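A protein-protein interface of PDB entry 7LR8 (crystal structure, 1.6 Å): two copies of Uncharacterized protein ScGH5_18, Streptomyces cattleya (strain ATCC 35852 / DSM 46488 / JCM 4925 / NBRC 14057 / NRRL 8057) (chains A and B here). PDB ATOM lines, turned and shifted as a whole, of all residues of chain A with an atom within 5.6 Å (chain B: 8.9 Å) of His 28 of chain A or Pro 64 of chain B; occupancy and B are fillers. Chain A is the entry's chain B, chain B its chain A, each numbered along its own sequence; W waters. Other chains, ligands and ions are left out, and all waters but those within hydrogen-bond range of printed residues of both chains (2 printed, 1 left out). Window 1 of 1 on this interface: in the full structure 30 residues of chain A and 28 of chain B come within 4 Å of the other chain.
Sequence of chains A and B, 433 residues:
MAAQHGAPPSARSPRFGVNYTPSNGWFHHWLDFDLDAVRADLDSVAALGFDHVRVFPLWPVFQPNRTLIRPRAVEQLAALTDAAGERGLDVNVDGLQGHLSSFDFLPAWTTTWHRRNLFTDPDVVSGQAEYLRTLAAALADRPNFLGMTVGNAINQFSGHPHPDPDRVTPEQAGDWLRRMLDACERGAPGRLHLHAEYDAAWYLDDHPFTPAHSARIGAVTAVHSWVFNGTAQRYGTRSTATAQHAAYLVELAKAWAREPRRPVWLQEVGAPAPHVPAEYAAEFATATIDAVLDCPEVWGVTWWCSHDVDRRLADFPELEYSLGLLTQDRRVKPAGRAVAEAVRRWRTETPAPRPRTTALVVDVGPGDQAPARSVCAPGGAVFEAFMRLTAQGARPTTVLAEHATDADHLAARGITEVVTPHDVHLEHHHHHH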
ATOM      1  N   GLY A  25     -21.585 -21.368   1.132  1.00  0.00           N
ATOM      2  CA  GLY A  25     -20.715 -21.056   0.013  1.00  0.00           C
ATOM      3  C   GLY A  25     -21.295 -21.319  -1.360  1.00  0.00           C
ATOM      4  O   GLY A  25     -20.678 -20.901  -2.355  1.00  0.00           O
ATOM      5  N   TRP A  26     -22.435 -22.002  -1.455  1.00  0.00           N
ATOM      6  CA  TRP A  26     -23.009 -22.346  -2.765  1.00  0.00           C
ATOM      7  C   TRP A  26     -21.941 -23.133  -3.532  1.00  0.00           C
ATOM      8  O   TRP A  26     -21.097 -23.811  -2.931  1.00  0.00           O
ATOM      9  CB  TRP A  26     -23.505 -21.070  -3.457  1.00  0.00           C
ATOM     10  CG  TRP A  26     -24.348 -21.270  -4.699  1.00  0.00           C
ATOM     11  CD1 TRP A  26     -25.591 -21.839  -4.768  1.00  0.00           C
ATOM     12  CD2 TRP A  26     -24.030 -20.841  -6.033  1.00  0.00           C
ATOM     13  NE1 TRP A  26     -26.053 -21.821  -6.061  1.00  0.00           N
ATOM     14  CE2 TRP A  26     -25.111 -21.219  -6.860  1.00  0.00           C
ATOM     15  CE3 TRP A  26     -22.920 -20.207  -6.611  1.00  0.00           C
ATOM     16  CZ2 TRP A  26     -25.127 -20.965  -8.231  1.00  0.00           C
ATOM     17  CZ3 TRP A  26     -22.932 -19.955  -7.984  1.00  0.00           C
ATOM     18  CH2 TRP A  26     -24.029 -20.337  -8.778  1.00  0.00           C
ATOM     19  N   PHE A  27     -21.944 -23.070  -4.858  1.00  0.00           N
ATOM     20  CA  PHE A  27     -20.928 -23.820  -5.593  1.00  0.00           C
ATOM     21  C   PHE A  27     -19.529 -23.252  -5.429  1.00  0.00           C
ATOM     22  O   PHE A  27     -18.562 -23.915  -5.832  1.00  0.00           O
ATOM     23  CB  PHE A  27     -21.311 -23.886  -7.060  1.00  0.00           C
ATOM     24  CG  PHE A  27     -22.628 -24.558  -7.287  1.00  0.00           C
ATOM     25  CD1 PHE A  27     -22.827 -25.872  -6.883  1.00  0.00           C
ATOM     26  CD2 PHE A  27     -23.665 -23.877  -7.889  1.00  0.00           C
ATOM     27  CE1 PHE A  27     -24.053 -26.492  -7.076  1.00  0.00           C
ATOM     28  CE2 PHE A  27     -24.893 -24.491  -8.094  1.00  0.00           C
ATOM     29  CZ  PHE A  27     -25.078 -25.808  -7.687  1.00  0.00           C
ATOM     30  N   HIS A  28     -19.392 -22.065  -4.837  1.00  0.00           N
ATOM     31  CA  HIS A  28     -18.071 -21.582  -4.471  1.00  0.00           C
ATOM     32  C   HIS A  28     -17.482 -22.344  -3.291  1.00  0.00           C
ATOM     33  O   HIS A  28     -16.358 -22.032  -2.877  1.00  0.00           O
ATOM     34  CB  HIS A  28     -18.115 -20.085  -4.155  1.00  0.00           C
ATOM     35  CG  HIS A  28     -18.806 -19.259  -5.201  1.00  0.00           C
ATOM     36  ND1 HIS A  28     -18.372 -19.194  -6.508  1.00  0.00           N
ATOM     37  CD2 HIS A  28     -19.888 -18.443  -5.121  1.00  0.00           C
ATOM     38  CE1 HIS A  28     -19.164 -18.387  -7.193  1.00  0.00           C
ATOM     39  NE2 HIS A  28     -20.092 -17.917  -6.376  1.00  0.00           N
ATOM     40  N   HIS A  29     -18.191 -23.344  -2.748  1.00  0.00           N
ATOM     41  CA  HIS A  29     -17.638 -24.082  -1.618  1.00  0.00           C
ATOM     42  C   HIS A  29     -16.370 -24.852  -1.993  1.00  0.00           C
ATOM     43  O   HIS A  29     -15.592 -25.202  -1.103  1.00  0.00           O
ATOM     44  CB  HIS A  29     -18.688 -25.027  -1.026  1.00  0.00           C
ATOM     45  CG  HIS A  29     -18.881 -26.293  -1.799  1.00  0.00           C
ATOM     46  ND1 HIS A  29     -18.898 -27.530  -1.193  1.00  0.00           N
ATOM     47  CD2 HIS A  29     -19.086 -26.517  -3.119  1.00  0.00           C
ATOM     48  CE1 HIS A  29     -19.088 -28.463  -2.107  1.00  0.00           C
ATOM     49  NE2 HIS A  29     -19.210 -27.877  -3.285  1.00  0.00           N
ATOM     50  N   TRP A  30     -16.117 -25.092  -3.281  1.00  0.00           N
ATOM     51  CA  TRP A  30     -14.845 -25.714  -3.646  1.00  0.00           C
ATOM     52  C   TRP A  30     -13.647 -24.870  -3.229  1.00  0.00           C
ATOM     53  O   TRP A  30     -12.543 -25.414  -3.074  1.00  0.00           O
ATOM     54  CB  TRP A  30     -14.783 -25.976  -5.141  1.00  0.00           C
ATOM     55  CG  TRP A  30     -15.880 -26.847  -5.655  1.00  0.00           C
ATOM     56  CD1 TRP A  30     -16.899 -26.466  -6.478  1.00  0.00           C
ATOM     57  CD2 TRP A  30     -16.078 -28.251  -5.388  1.00  0.00           C
ATOM     58  NE1 TRP A  30     -17.714 -27.537  -6.746  1.00  0.00           N
ATOM     59  CE2 TRP A  30     -17.238 -28.644  -6.088  1.00  0.00           C
ATOM     60  CE3 TRP A  30     -15.382 -29.211  -4.639  1.00  0.00           C
ATOM     61  CZ2 TRP A  30     -17.727 -29.958  -6.059  1.00  0.00           C
ATOM     62  CZ3 TRP A  30     -15.880 -30.526  -4.602  1.00  0.00           C
ATOM     63  CH2 TRP A  30     -17.040 -30.880  -5.312  1.00  0.00           C
ATOM     64  N   LEU A  31     -13.838 -23.557  -3.049  1.00  0.00           N
ATOM     65  CA  LEU A  31     -12.760 -22.678  -2.613  1.00  0.00           C
ATOM     66  C   LEU A  31     -12.559 -22.684  -1.107  1.00  0.00           C
ATOM     67  O   LEU A  31     -11.530 -22.181  -0.635  1.00  0.00           O
ATOM     68  CB  LEU A  31     -13.025 -21.241  -3.084  1.00  0.00           C
ATOM     69  CG  LEU A  31     -13.218 -21.052  -4.590  1.00  0.00           C
ATOM     70  CD1 LEU A  31     -13.632 -19.604  -4.880  1.00  0.00           C
ATOM     71  CD2 LEU A  31     -11.948 -21.396  -5.364  1.00  0.00           C
ATOM     72  N   ASP A  32     -13.510 -23.222  -0.350  1.00  0.00           N
ATOM     73  CA  ASP A  32     -13.478 -23.257   1.106  1.00  0.00           C
ATOM     74  C   ASP A  32     -14.130 -24.568   1.520  1.00  0.00           C
ATOM     75  O   ASP A  32     -15.167 -24.605   2.205  1.00  0.00           O
ATOM     76  CB  ASP A  32     -14.192 -22.050   1.710  1.00  0.00           C
ATOM     77  CG  ASP A  32     -13.502 -20.738   1.373  1.00  0.00           C
ATOM     78  OD1 ASP A  32     -12.407 -20.473   1.928  1.00  0.00           O
ATOM     79  OD2 ASP A  32     -14.049 -19.992   0.537  1.00  0.00           O
ATOM     80  N   LEU A  58     -17.080 -26.782 -10.234  1.00  0.00           N
ATOM     81  CA  LEU A  58     -16.898 -25.546 -10.992  1.00  0.00           C
ATOM     82  C   LEU A  58     -15.690 -25.765 -11.899  1.00  0.00           C
ATOM     83  O   LEU A  58     -14.562 -25.907 -11.415  1.00  0.00           O
ATOM     84  CB  LEU A  58     -16.684 -24.348 -10.077  1.00  0.00           C
ATOM     85  CG  LEU A  58     -17.924 -23.795  -9.373  1.00  0.00           C
ATOM     86  CD1 LEU A  58     -17.580 -22.529  -8.604  1.00  0.00           C
ATOM     87  CD2 LEU A  58     -19.039 -23.530 -10.371  1.00  0.00           C
ATOM     88  N   PHE A 105     -19.319 -19.801 -15.792  1.00  0.00           N
ATOM     89  CA  PHE A 105     -17.998 -20.024 -15.200  1.00  0.00           C
ATOM     90  C   PHE A 105     -17.090 -20.566 -16.298  1.00  0.00           C
ATOM     91  O   PHE A 105     -17.063 -21.773 -16.558  1.00  0.00           O
ATOM     92  CB  PHE A 105     -18.100 -20.969 -14.005  1.00  0.00           C
ATOM     93  CG  PHE A 105     -18.904 -20.390 -12.869  1.00  0.00           C
ATOM     94  CD1 PHE A 105     -18.332 -19.489 -11.988  1.00  0.00           C
ATOM     95  CD2 PHE A 105     -20.247 -20.693 -12.737  1.00  0.00           C
ATOM     96  CE1 PHE A 105     -19.078 -18.907 -10.956  1.00  0.00           C
ATOM     97  CE2 PHE A 105     -21.001 -20.128 -11.711  1.00  0.00           C
ATOM     98  CZ  PHE A 105     -20.411 -19.235 -10.821  1.00  0.00           C
ATOM     99  N   LEU A 313     -25.323 -13.490  -1.068  1.00  0.00           N
ATOM    100  CA  LEU A 313     -24.669 -13.573  -2.370  1.00  0.00           C
ATOM    101  C   LEU A 313     -25.474 -12.724  -3.347  1.00  0.00           C
ATOM    102  O   LEU A 313     -26.703 -12.831  -3.399  1.00  0.00           O
ATOM    103  CB  LEU A 313     -24.576 -15.020  -2.847  1.00  0.00           C
ATOM    104  CG  LEU A 313     -23.714 -15.987  -2.027  1.00  0.00           C
ATOM    105  CD1 LEU A 313     -23.980 -17.419  -2.454  1.00  0.00           C
ATOM    106  CD2 LEU A 313     -22.228 -15.662  -2.186  1.00  0.00           C
ATOM    107  N   LEU B  31      -5.386 -21.424  -5.009  1.00  0.00           N
ATOM    108  CA  LEU B  31      -6.272 -22.580  -4.889  1.00  0.00           C
ATOM    109  C   LEU B  31      -5.629 -23.750  -4.161  1.00  0.00           C
ATOM    110  O   LEU B  31      -6.327 -24.705  -3.815  1.00  0.00           O
ATOM    111  CB  LEU B  31      -6.715 -23.064  -6.272  1.00  0.00           C
ATOM    112  CG  LEU B  31      -7.367 -22.040  -7.190  1.00  0.00           C
ATOM    113  CD1 LEU B  31      -7.535 -22.597  -8.595  1.00  0.00           C
ATOM    114  CD2 LEU B  31      -8.707 -21.609  -6.589  1.00  0.00           C
ATOM    115  N   LEU B  58      -5.558 -13.240  -7.247  1.00  0.00           N
ATOM    116  CA  LEU B  58      -6.415 -13.468  -8.408  1.00  0.00           C
ATOM    117  C   LEU B  58      -7.818 -13.015  -8.018  1.00  0.00           C
ATOM    118  O   LEU B  58      -8.448 -13.607  -7.130  1.00  0.00           O
ATOM    119  CB  LEU B  58      -6.415 -14.938  -8.836  1.00  0.00           C
ATOM    120  CG  LEU B  58      -5.242 -15.426  -9.681  1.00  0.00           C
ATOM    121  CD1 LEU B  58      -5.533 -16.819 -10.211  1.00  0.00           C
ATOM    122  CD2 LEU B  58      -4.988 -14.440 -10.820  1.00  0.00           C
ATOM    123  N   TRP B  59      -8.296 -11.963  -8.679  1.00  0.00           N
ATOM    124  CA  TRP B  59      -9.542 -11.301  -8.285  1.00  0.00           C
ATOM    125  C   TRP B  59     -10.741 -12.241  -8.203  1.00  0.00           C
ATOM    126  O   TRP B  59     -11.419 -12.244  -7.160  1.00  0.00           O
ATOM    127  CB  TRP B  59      -9.785 -10.128  -9.248  1.00  0.00           C
ATOM    128  CG  TRP B  59     -11.050  -9.332  -8.978  1.00  0.00           C
ATOM    129  CD1 TRP B  59     -11.694  -9.171  -7.780  1.00  0.00           C
ATOM    130  CD2 TRP B  59     -11.799  -8.582  -9.943  1.00  0.00           C
ATOM    131  NE1 TRP B  59     -12.812  -8.373  -7.948  1.00  0.00           N
ATOM    132  CE2 TRP B  59     -12.897  -8.005  -9.267  1.00  0.00           C
ATOM    133  CE3 TRP B  59     -11.655  -8.357 -11.318  1.00  0.00           C
ATOM    134  CZ2 TRP B  59     -13.838  -7.206  -9.919  1.00  0.00           C
ATOM    135  CZ3 TRP B  59     -12.596  -7.569 -11.967  1.00  0.00           C
ATOM    136  CH2 TRP B  59     -13.669  -6.993 -11.263  1.00  0.00           C
ATOM    137  N   PRO B  60     -11.060 -13.063  -9.214  1.00  0.00           N
ATOM    138  CA  PRO B  60     -12.231 -13.949  -9.063  1.00  0.00           C
ATOM    139  C   PRO B  60     -12.066 -15.028  -7.998  1.00  0.00           C
ATOM    140  O   PRO B  60     -13.080 -15.538  -7.509  1.00  0.00           O
ATOM    141  CB  PRO B  60     -12.412 -14.558 -10.458  1.00  0.00           C
ATOM    142  CG  PRO B  60     -11.134 -14.293 -11.189  1.00  0.00           C
ATOM    143  CD  PRO B  60     -10.454 -13.154 -10.559  1.00  0.00           C
ATOM    144  N   VAL B  61     -10.834 -15.395  -7.629  1.00  0.00           N
ATOM    145  CA  VAL B  61     -10.631 -16.343  -6.533  1.00  0.00           C
ATOM    146  C   VAL B  61     -10.898 -15.664  -5.194  1.00  0.00           C
ATOM    147  O   VAL B  61     -11.461 -16.269  -4.269  1.00  0.00           O
ATOM    148  CB  VAL B  61      -9.210 -16.927  -6.609  1.00  0.00           C
ATOM    149  CG1 VAL B  61      -8.875 -17.727  -5.355  1.00  0.00           C
ATOM    150  CG2 VAL B  61      -9.068 -17.788  -7.853  1.00  0.00           C
ATOM    151  N   PHE B  62     -10.517 -14.392  -5.080  1.00  0.00           N
ATOM    152  CA  PHE B  62     -10.716 -13.653  -3.841  1.00  0.00           C
ATOM    153  C   PHE B  62     -12.147 -13.155  -3.694  1.00  0.00           C
ATOM    154  O   PHE B  62     -12.645 -13.056  -2.566  1.00  0.00           O
ATOM    155  CB  PHE B  62      -9.746 -12.462  -3.777  1.00  0.00           C
ATOM    156  CG  PHE B  62      -8.364 -12.814  -3.257  1.00  0.00           C
ATOM    157  CD1 PHE B  62      -7.584 -13.767  -3.891  1.00  0.00           C
ATOM    158  CD2 PHE B  62      -7.854 -12.179  -2.124  1.00  0.00           C
ATOM    159  CE1 PHE B  62      -6.317 -14.090  -3.415  1.00  0.00           C
ATOM    160  CE2 PHE B  62      -6.579 -12.497  -1.641  1.00  0.00           C
ATOM    161  CZ  PHE B  62      -5.817 -13.464  -2.290  1.00  0.00           C
ATOM    162  N   GLN B  63     -12.814 -12.823  -4.805  1.00  0.00           N
ATOM    163  CA  GLN B  63     -14.163 -12.239  -4.791  1.00  0.00           C
ATOM    164  C   GLN B  63     -15.030 -12.989  -5.793  1.00  0.00           C
ATOM    165  O   GLN B  63     -15.367 -12.459  -6.858  1.00  0.00           O
ATOM    166  CB  GLN B  63     -14.110 -10.743  -5.116  1.00  0.00           C
ATOM    167  CG  GLN B  63     -15.443 -10.026  -4.898  1.00  0.00           C
ATOM    168  CD  GLN B  63     -15.330  -8.508  -5.049  1.00  0.00           C
ATOM    169  OE1 GLN B  63     -14.436  -8.002  -5.738  1.00  0.00           O
ATOM    170  NE2 GLN B  63     -16.222  -7.781  -4.383  1.00  0.00           N
ATOM    171  N   PRO B  64     -15.360 -14.257  -5.509  1.00  0.00           N
ATOM    172  CA  PRO B  64     -16.077 -15.063  -6.511  1.00  0.00           C
ATOM    173  C   PRO B  64     -17.508 -14.614  -6.751  1.00  0.00           C
ATOM    174  O   PRO B  64     -18.096 -14.993  -7.770  1.00  0.00           O
ATOM    175  CB  PRO B  64     -16.034 -16.481  -5.914  1.00  0.00           C
ATOM    176  CG  PRO B  64     -15.923 -16.278  -4.431  1.00  0.00           C
ATOM    177  CD  PRO B  64     -15.040 -15.041  -4.298  1.00  0.00           C
ATOM    178  N   ASN B  65     -18.083 -13.849  -5.831  1.00  0.00           N
ATOM    179  CA  ASN B  65     -19.385 -13.220  -5.969  1.00  0.00           C
ATOM    180  C   ASN B  65     -19.198 -11.767  -5.547  1.00  0.00           C
ATOM    181  O   ASN B  65     -18.308 -11.469  -4.750  1.00  0.00           O
ATOM    182  CB  ASN B  65     -20.423 -13.956  -5.100  1.00  0.00           C
ATOM    183  CG  ASN B  65     -21.783 -13.300  -5.110  1.00  0.00           C
ATOM    184  OD1 ASN B  65     -22.015 -12.332  -4.384  1.00  0.00           O
ATOM    185  ND2 ASN B  65     -22.703 -13.841  -5.907  1.00  0.00           N
ATOM    186  N   ARG B  66     -19.997 -10.855  -6.118  1.00  0.00           N
ATOM    187  CA  ARG B  66     -19.807  -9.437  -5.819  1.00  0.00           C
ATOM    188  C   ARG B  66     -19.811  -9.158  -4.319  1.00  0.00           C
ATOM    189  O   ARG B  66     -19.063  -8.294  -3.851  1.00  0.00           O
ATOM    190  CB  ARG B  66     -20.874  -8.589  -6.521  1.00  0.00           C
ATOM    191  CG  ARG B  66     -20.740  -7.086  -6.261  1.00  0.00           C
ATOM    192  CD  ARG B  66     -21.582  -6.272  -7.225  1.00  0.00           C
ATOM    193  NE  ARG B  66     -23.008  -6.617  -7.247  1.00  0.00           N
ATOM    194  CZ  ARG B  66     -23.941  -6.043  -6.480  1.00  0.00           C
ATOM    195  NH1 ARG B  66     -23.599  -5.108  -5.604  1.00  0.00           N
ATOM    196  NH2 ARG B  66     -25.222  -6.388  -6.586  1.00  0.00           N
ATOM    197  N   THR B  67     -20.602  -9.893  -3.537  1.00  0.00           N
ATOM    198  CA  THR B  67     -20.635  -9.657  -2.097  1.00  0.00           C
ATOM    199  C   THR B  67     -20.136 -10.874  -1.321  1.00  0.00           C
ATOM    200  O   THR B  67     -20.634 -11.208  -0.245  1.00  0.00           O
ATOM    201  CB  THR B  67     -22.029  -9.229  -1.634  1.00  0.00           C
ATOM    202  OG1 THR B  67     -23.020 -10.171  -2.079  1.00  0.00           O
ATOM    203  CG2 THR B  67     -22.350  -7.850  -2.187  1.00  0.00           C
ATOM    204  N   LEU B  68     -19.113 -11.539  -1.851  1.00  0.00           N
ATOM    205  CA  LEU B  68     -18.382 -12.554  -1.099  1.00  0.00           C
ATOM    206  C   LEU B  68     -16.902 -12.299  -1.354  1.00  0.00           C
ATOM    207  O   LEU B  68     -16.370 -12.677  -2.404  1.00  0.00           O
ATOM    208  CB  LEU B  68     -18.773 -13.971  -1.499  1.00  0.00           C
ATOM    209  CG  LEU B  68     -17.870 -15.081  -0.936  1.00  0.00           C
ATOM    210  CD1 LEU B  68     -17.780 -15.014   0.579  1.00  0.00           C
ATOM    211  CD2 LEU B  68     -18.362 -16.453  -1.363  1.00  0.00           C
ATOM    212  N   ILE B  69     -16.256 -11.628  -0.405  1.00  0.00           N
ATOM    213  CA  ILE B  69     -14.804 -11.507  -0.383  1.00  0.00           C
ATOM    214  C   ILE B  69     -14.301 -12.520   0.635  1.00  0.00           C
ATOM    215  O   ILE B  69     -14.562 -12.391   1.835  1.00  0.00           O
ATOM    216  CB  ILE B  69     -14.354 -10.084  -0.040  1.00  0.00           C
ATOM    217  CG1 ILE B  69     -14.906  -9.112  -1.077  1.00  0.00           C
ATOM    218  CG2 ILE B  69     -12.828 -10.025   0.049  1.00  0.00           C
ATOM    219  CD1 ILE B  69     -14.983  -7.686  -0.583  1.00  0.00           C
ATOM    220  N   ARG B  70     -13.587 -13.540   0.157  1.00  0.00           N
ATOM    221  CA  ARG B  70     -13.319 -14.718   0.979  1.00  0.00           C
ATOM    222  C   ARG B  70     -12.304 -14.413   2.076  1.00  0.00           C
ATOM    223  O   ARG B  70     -11.149 -14.077   1.766  1.00  0.00           O
ATOM    224  CB  ARG B  70     -12.816 -15.854   0.093  1.00  0.00           C
ATOM    225  CG  ARG B  70     -13.859 -16.397  -0.884  1.00  0.00           C
ATOM    226  CD  ARG B  70     -13.254 -17.485  -1.774  1.00  0.00           C
ATOM    227  NE  ARG B  70     -12.446 -18.396  -0.966  1.00  0.00           N
ATOM    228  CZ  ARG B  70     -11.140 -18.600  -1.113  1.00  0.00           C
ATOM    229  NH1 ARG B  70     -10.456 -17.984  -2.074  1.00  0.00           N
ATOM    230  NH2 ARG B  70     -10.517 -19.434  -0.290  1.00  0.00           N
ATOM    231  N   PRO B  71     -12.673 -14.531   3.355  1.00  0.00           N
ATOM    232  CA  PRO B  71     -11.698 -14.262   4.425  1.00  0.00           C
ATOM    233  C   PRO B  71     -10.473 -15.160   4.395  1.00  0.00           C
ATOM    234  O   PRO B  71      -9.390 -14.712   4.787  1.00  0.00           O
ATOM    235  CB  PRO B  71     -12.511 -14.479   5.705  1.00  0.00           C
ATOM    236  CG  PRO B  71     -13.930 -14.324   5.298  1.00  0.00           C
ATOM    237  CD  PRO B  71     -14.032 -14.757   3.878  1.00  0.00           C
ATOM    238  N   ALA B  73      -8.900 -16.248   1.749  1.00  0.00           N
ATOM    239  CA  ALA B  73      -7.978 -15.709   0.757  1.00  0.00           C
ATOM    240  C   ALA B  73      -7.248 -14.498   1.317  1.00  0.00           C
ATOM    241  O   ALA B  73      -6.043 -14.342   1.112  1.00  0.00           O
ATOM    242  CB  ALA B  73      -8.730 -15.356  -0.522  1.00  0.00           C
ATOM    243  N   LEU B 106     -11.524 -12.856 -14.975  1.00  0.00           N
ATOM    244  CA  LEU B 106     -12.683 -12.010 -14.781  1.00  0.00           C
ATOM    245  C   LEU B 106     -13.729 -12.758 -13.973  1.00  0.00           C
ATOM    246  O   LEU B 106     -14.021 -13.926 -14.272  1.00  0.00           O
ATOM    247  CB  LEU B 106     -13.259 -11.586 -16.136  1.00  0.00           C
ATOM    248  CG  LEU B 106     -12.376 -10.619 -16.936  1.00  0.00           C
ATOM    249  CD1 LEU B 106     -12.839 -10.529 -18.382  1.00  0.00           C
ATOM    250  CD2 LEU B 106     -12.347  -9.241 -16.266  1.00  0.00           C
ATOM    251  N   PRO B 107     -14.297 -12.150 -12.931  1.00  0.00           N
ATOM    252  CA  PRO B 107     -15.338 -12.842 -12.162  1.00  0.00           C
ATOM    253  C   PRO B 107     -16.569 -13.096 -13.015  1.00  0.00           C
ATOM    254  O   PRO B 107     -16.903 -12.317 -13.908  1.00  0.00           O
ATOM    255  CB  PRO B 107     -15.636 -11.878 -11.010  1.00  0.00           C
ATOM    256  CG  PRO B 107     -14.432 -10.972 -10.943  1.00  0.00           C
ATOM    257  CD  PRO B 107     -13.943 -10.842 -12.355  1.00  0.00           C
ATOM    258  N   ALA B 108     -17.235 -14.221 -12.739  1.00  0.00           N
ATOM    259  CA  ALA B 108     -18.426 -14.569 -13.503  1.00  0.00           C
ATOM    260  C   ALA B 108     -19.503 -13.498 -13.380  1.00  0.00           C
ATOM    261  O   ALA B 108     -20.317 -13.336 -14.296  1.00  0.00           O
ATOM    262  CB  ALA B 108     -18.981 -15.914 -13.051  1.00  0.00           C
ATOM    263  N   TRP B 109     -19.510 -12.747 -12.282  1.00  0.00           N
ATOM    264  CA  TRP B 109     -20.499 -11.686 -12.111  1.00  0.00           C
ATOM    265  C   TRP B 109     -20.164 -10.417 -12.920  1.00  0.00           C
ATOM    266  O   TRP B 109     -20.863  -9.405 -12.770  1.00  0.00           O
ATOM    267  CB  TRP B 109     -20.681 -11.357 -10.613  1.00  0.00           C
ATOM    268  CG  TRP B 109     -19.417 -11.141  -9.789  1.00  0.00           C
ATOM    269  CD1 TRP B 109     -18.650 -12.097  -9.193  1.00  0.00           C
ATOM    270  CD2 TRP B 109     -18.804  -9.876  -9.463  1.00  0.00           C
ATOM    271  NE1 TRP B 109     -17.595 -11.510  -8.521  1.00  0.00           N
ATOM    272  CE2 TRP B 109     -17.661 -10.155  -8.681  1.00  0.00           C
ATOM    273  CE3 TRP B 109     -19.110  -8.536  -9.769  1.00  0.00           C
ATOM    274  CZ2 TRP B 109     -16.824  -9.148  -8.188  1.00  0.00           C
ATOM    275  CZ3 TRP B 109     -18.279  -7.533  -9.276  1.00  0.00           C
ATOM    276  CH2 TRP B 109     -17.137  -7.851  -8.506  1.00  0.00           C
ATOM    277  N   THR B 110     -19.152 -10.457 -13.794  1.00  0.00           N
ATOM    278  CA  THR B 110     -18.866  -9.337 -14.690  1.00  0.00           C
ATOM    279  C   THR B 110     -19.043  -9.669 -16.166  1.00  0.00           C
ATOM    280  O   THR B 110     -18.902  -8.767 -17.001  1.00  0.00           O
ATOM    281  CB  THR B 110     -17.438  -8.787 -14.489  1.00  0.00           C
ATOM    282  OG1 THR B 110     -16.444  -9.725 -14.961  1.00  0.00           O
ATOM    283  CG2 THR B 110     -17.185  -8.411 -13.023  1.00  0.00           C
ATOM    284  N   TYR B 131     -13.615  -4.619  -2.271  1.00  0.00           N
ATOM    285  CA  TYR B 131     -12.514  -5.575  -2.382  1.00  0.00           C
ATOM    286  C   TYR B 131     -11.180  -4.919  -2.031  1.00  0.00           C
ATOM    287  O   TYR B 131     -10.442  -5.408  -1.168  1.00  0.00           O
ATOM    288  CB  TYR B 131     -12.497  -6.158  -3.801  1.00  0.00           C
ATOM    289  CG  TYR B 131     -11.264  -6.937  -4.211  1.00  0.00           C
ATOM    290  CD1 TYR B 131     -10.985  -8.191  -3.673  1.00  0.00           C
ATOM    291  CD2 TYR B 131     -10.406  -6.433  -5.182  1.00  0.00           C
ATOM    292  CE1 TYR B 131      -9.859  -8.904  -4.062  1.00  0.00           C
ATOM    293  CE2 TYR B 131      -9.284  -7.144  -5.585  1.00  0.00           C
ATOM    294  CZ  TYR B 131      -9.022  -8.381  -5.028  1.00  0.00           C
ATOM    295  OH  TYR B 131      -7.905  -9.081  -5.425  1.00  0.00           O
HETATM  296  O   HOH W   1      -9.300 -21.909  -2.207  1.00  0.00           O
HETATM  297  O   HOH W   2     -22.140 -16.256  -7.370  1.00  0.00           O
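His 28 of chain A touches Pro 64 of chain B. Leu 31 of chain A touches Leu 31 of chain B (CD2 to CD2, 3.5 Å). Phe 105 of chain A touches Ala 108 of chain B (CE1 to CB, 3.7 Å). CA of Leu 313 of chain A touches OD1 of Asn 65 of chain B, at 3.6 Å. C of Leu 313 of chain A touches OG1 of Thr 67 of chain B (3.8 Å). Leu 68 of chain B touches Leu 313 of chain A (CB to CD2, 3.9 Å).
NH2 of Arg 70 of chain B is in hydrogen-bond range of O of Leu 31 of chain A, 2.9 Å away. NE of Arg 70 of chain B is in salt-bridge range of OD2 of Asp 32 of chain A (2.7 Å).
His 28 of chain A touches just one residue of chain B: Pro 64. Of the printed residues of chain A, Leu 31 of chain B touches Leu 31. Of chain A, only His 28 comes within 4 Å of Pro 64 of chain B. Printed residues of chain A within 4 Å of Arg 70 of chain B: Leu 31 (2.9 Å) and Asp 32 (2.7 Å). Of the printed residues of chain A, Ala 108 of chain B touches Phe 105. The nearest residue of chain B that does not touch His 28 of chain A is Asn 65 of chain B (4.2 Å). The nearest printed residue of chain A that does not touch Asn 65 of chain B is His 28 of chain A (4.2 Å).
Among the printed residues, 8 pairs touch across the chains. Among the printed residues, Asp or Glu carboxylates within 4 Å of a Lys or Arg side-chain nitrogen of the other chain: Asp 32 of chain A with Arg 70 of chain B.
The guanidinium group (NH1) of Arg 70 of chain B lies within hydrogen-bond range of the backbone carbonyl oxygen (O) of Val 61 of chain B (3.0 Å). The backbone NH of Arg 70 of chain B sits at hydrogen-bond distance from the backbone carbonyl oxygen of Phe 62 of chain B. The backbone NH of Thr 67 of chain B sits at hydrogen-bond distance from the side-chain amide oxygen of Asn 65 of chain B.
Water W1 bridges the backbone carbonyl oxygen of Leu 31 of chain A (2.7 Å) and the guanidinium group of Arg 70 of chain B (3.4 Å). Water W2 bridges NE2 of His 28 of chain A and ND2 of Asn 65 of chain B.
Leu 31 of chain B touches its own counterpart, Leu 31 of chain A. Of the 8 pairs that touch across the chains among the printed residues, 1 has its exchanged pair printed and touching as well.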
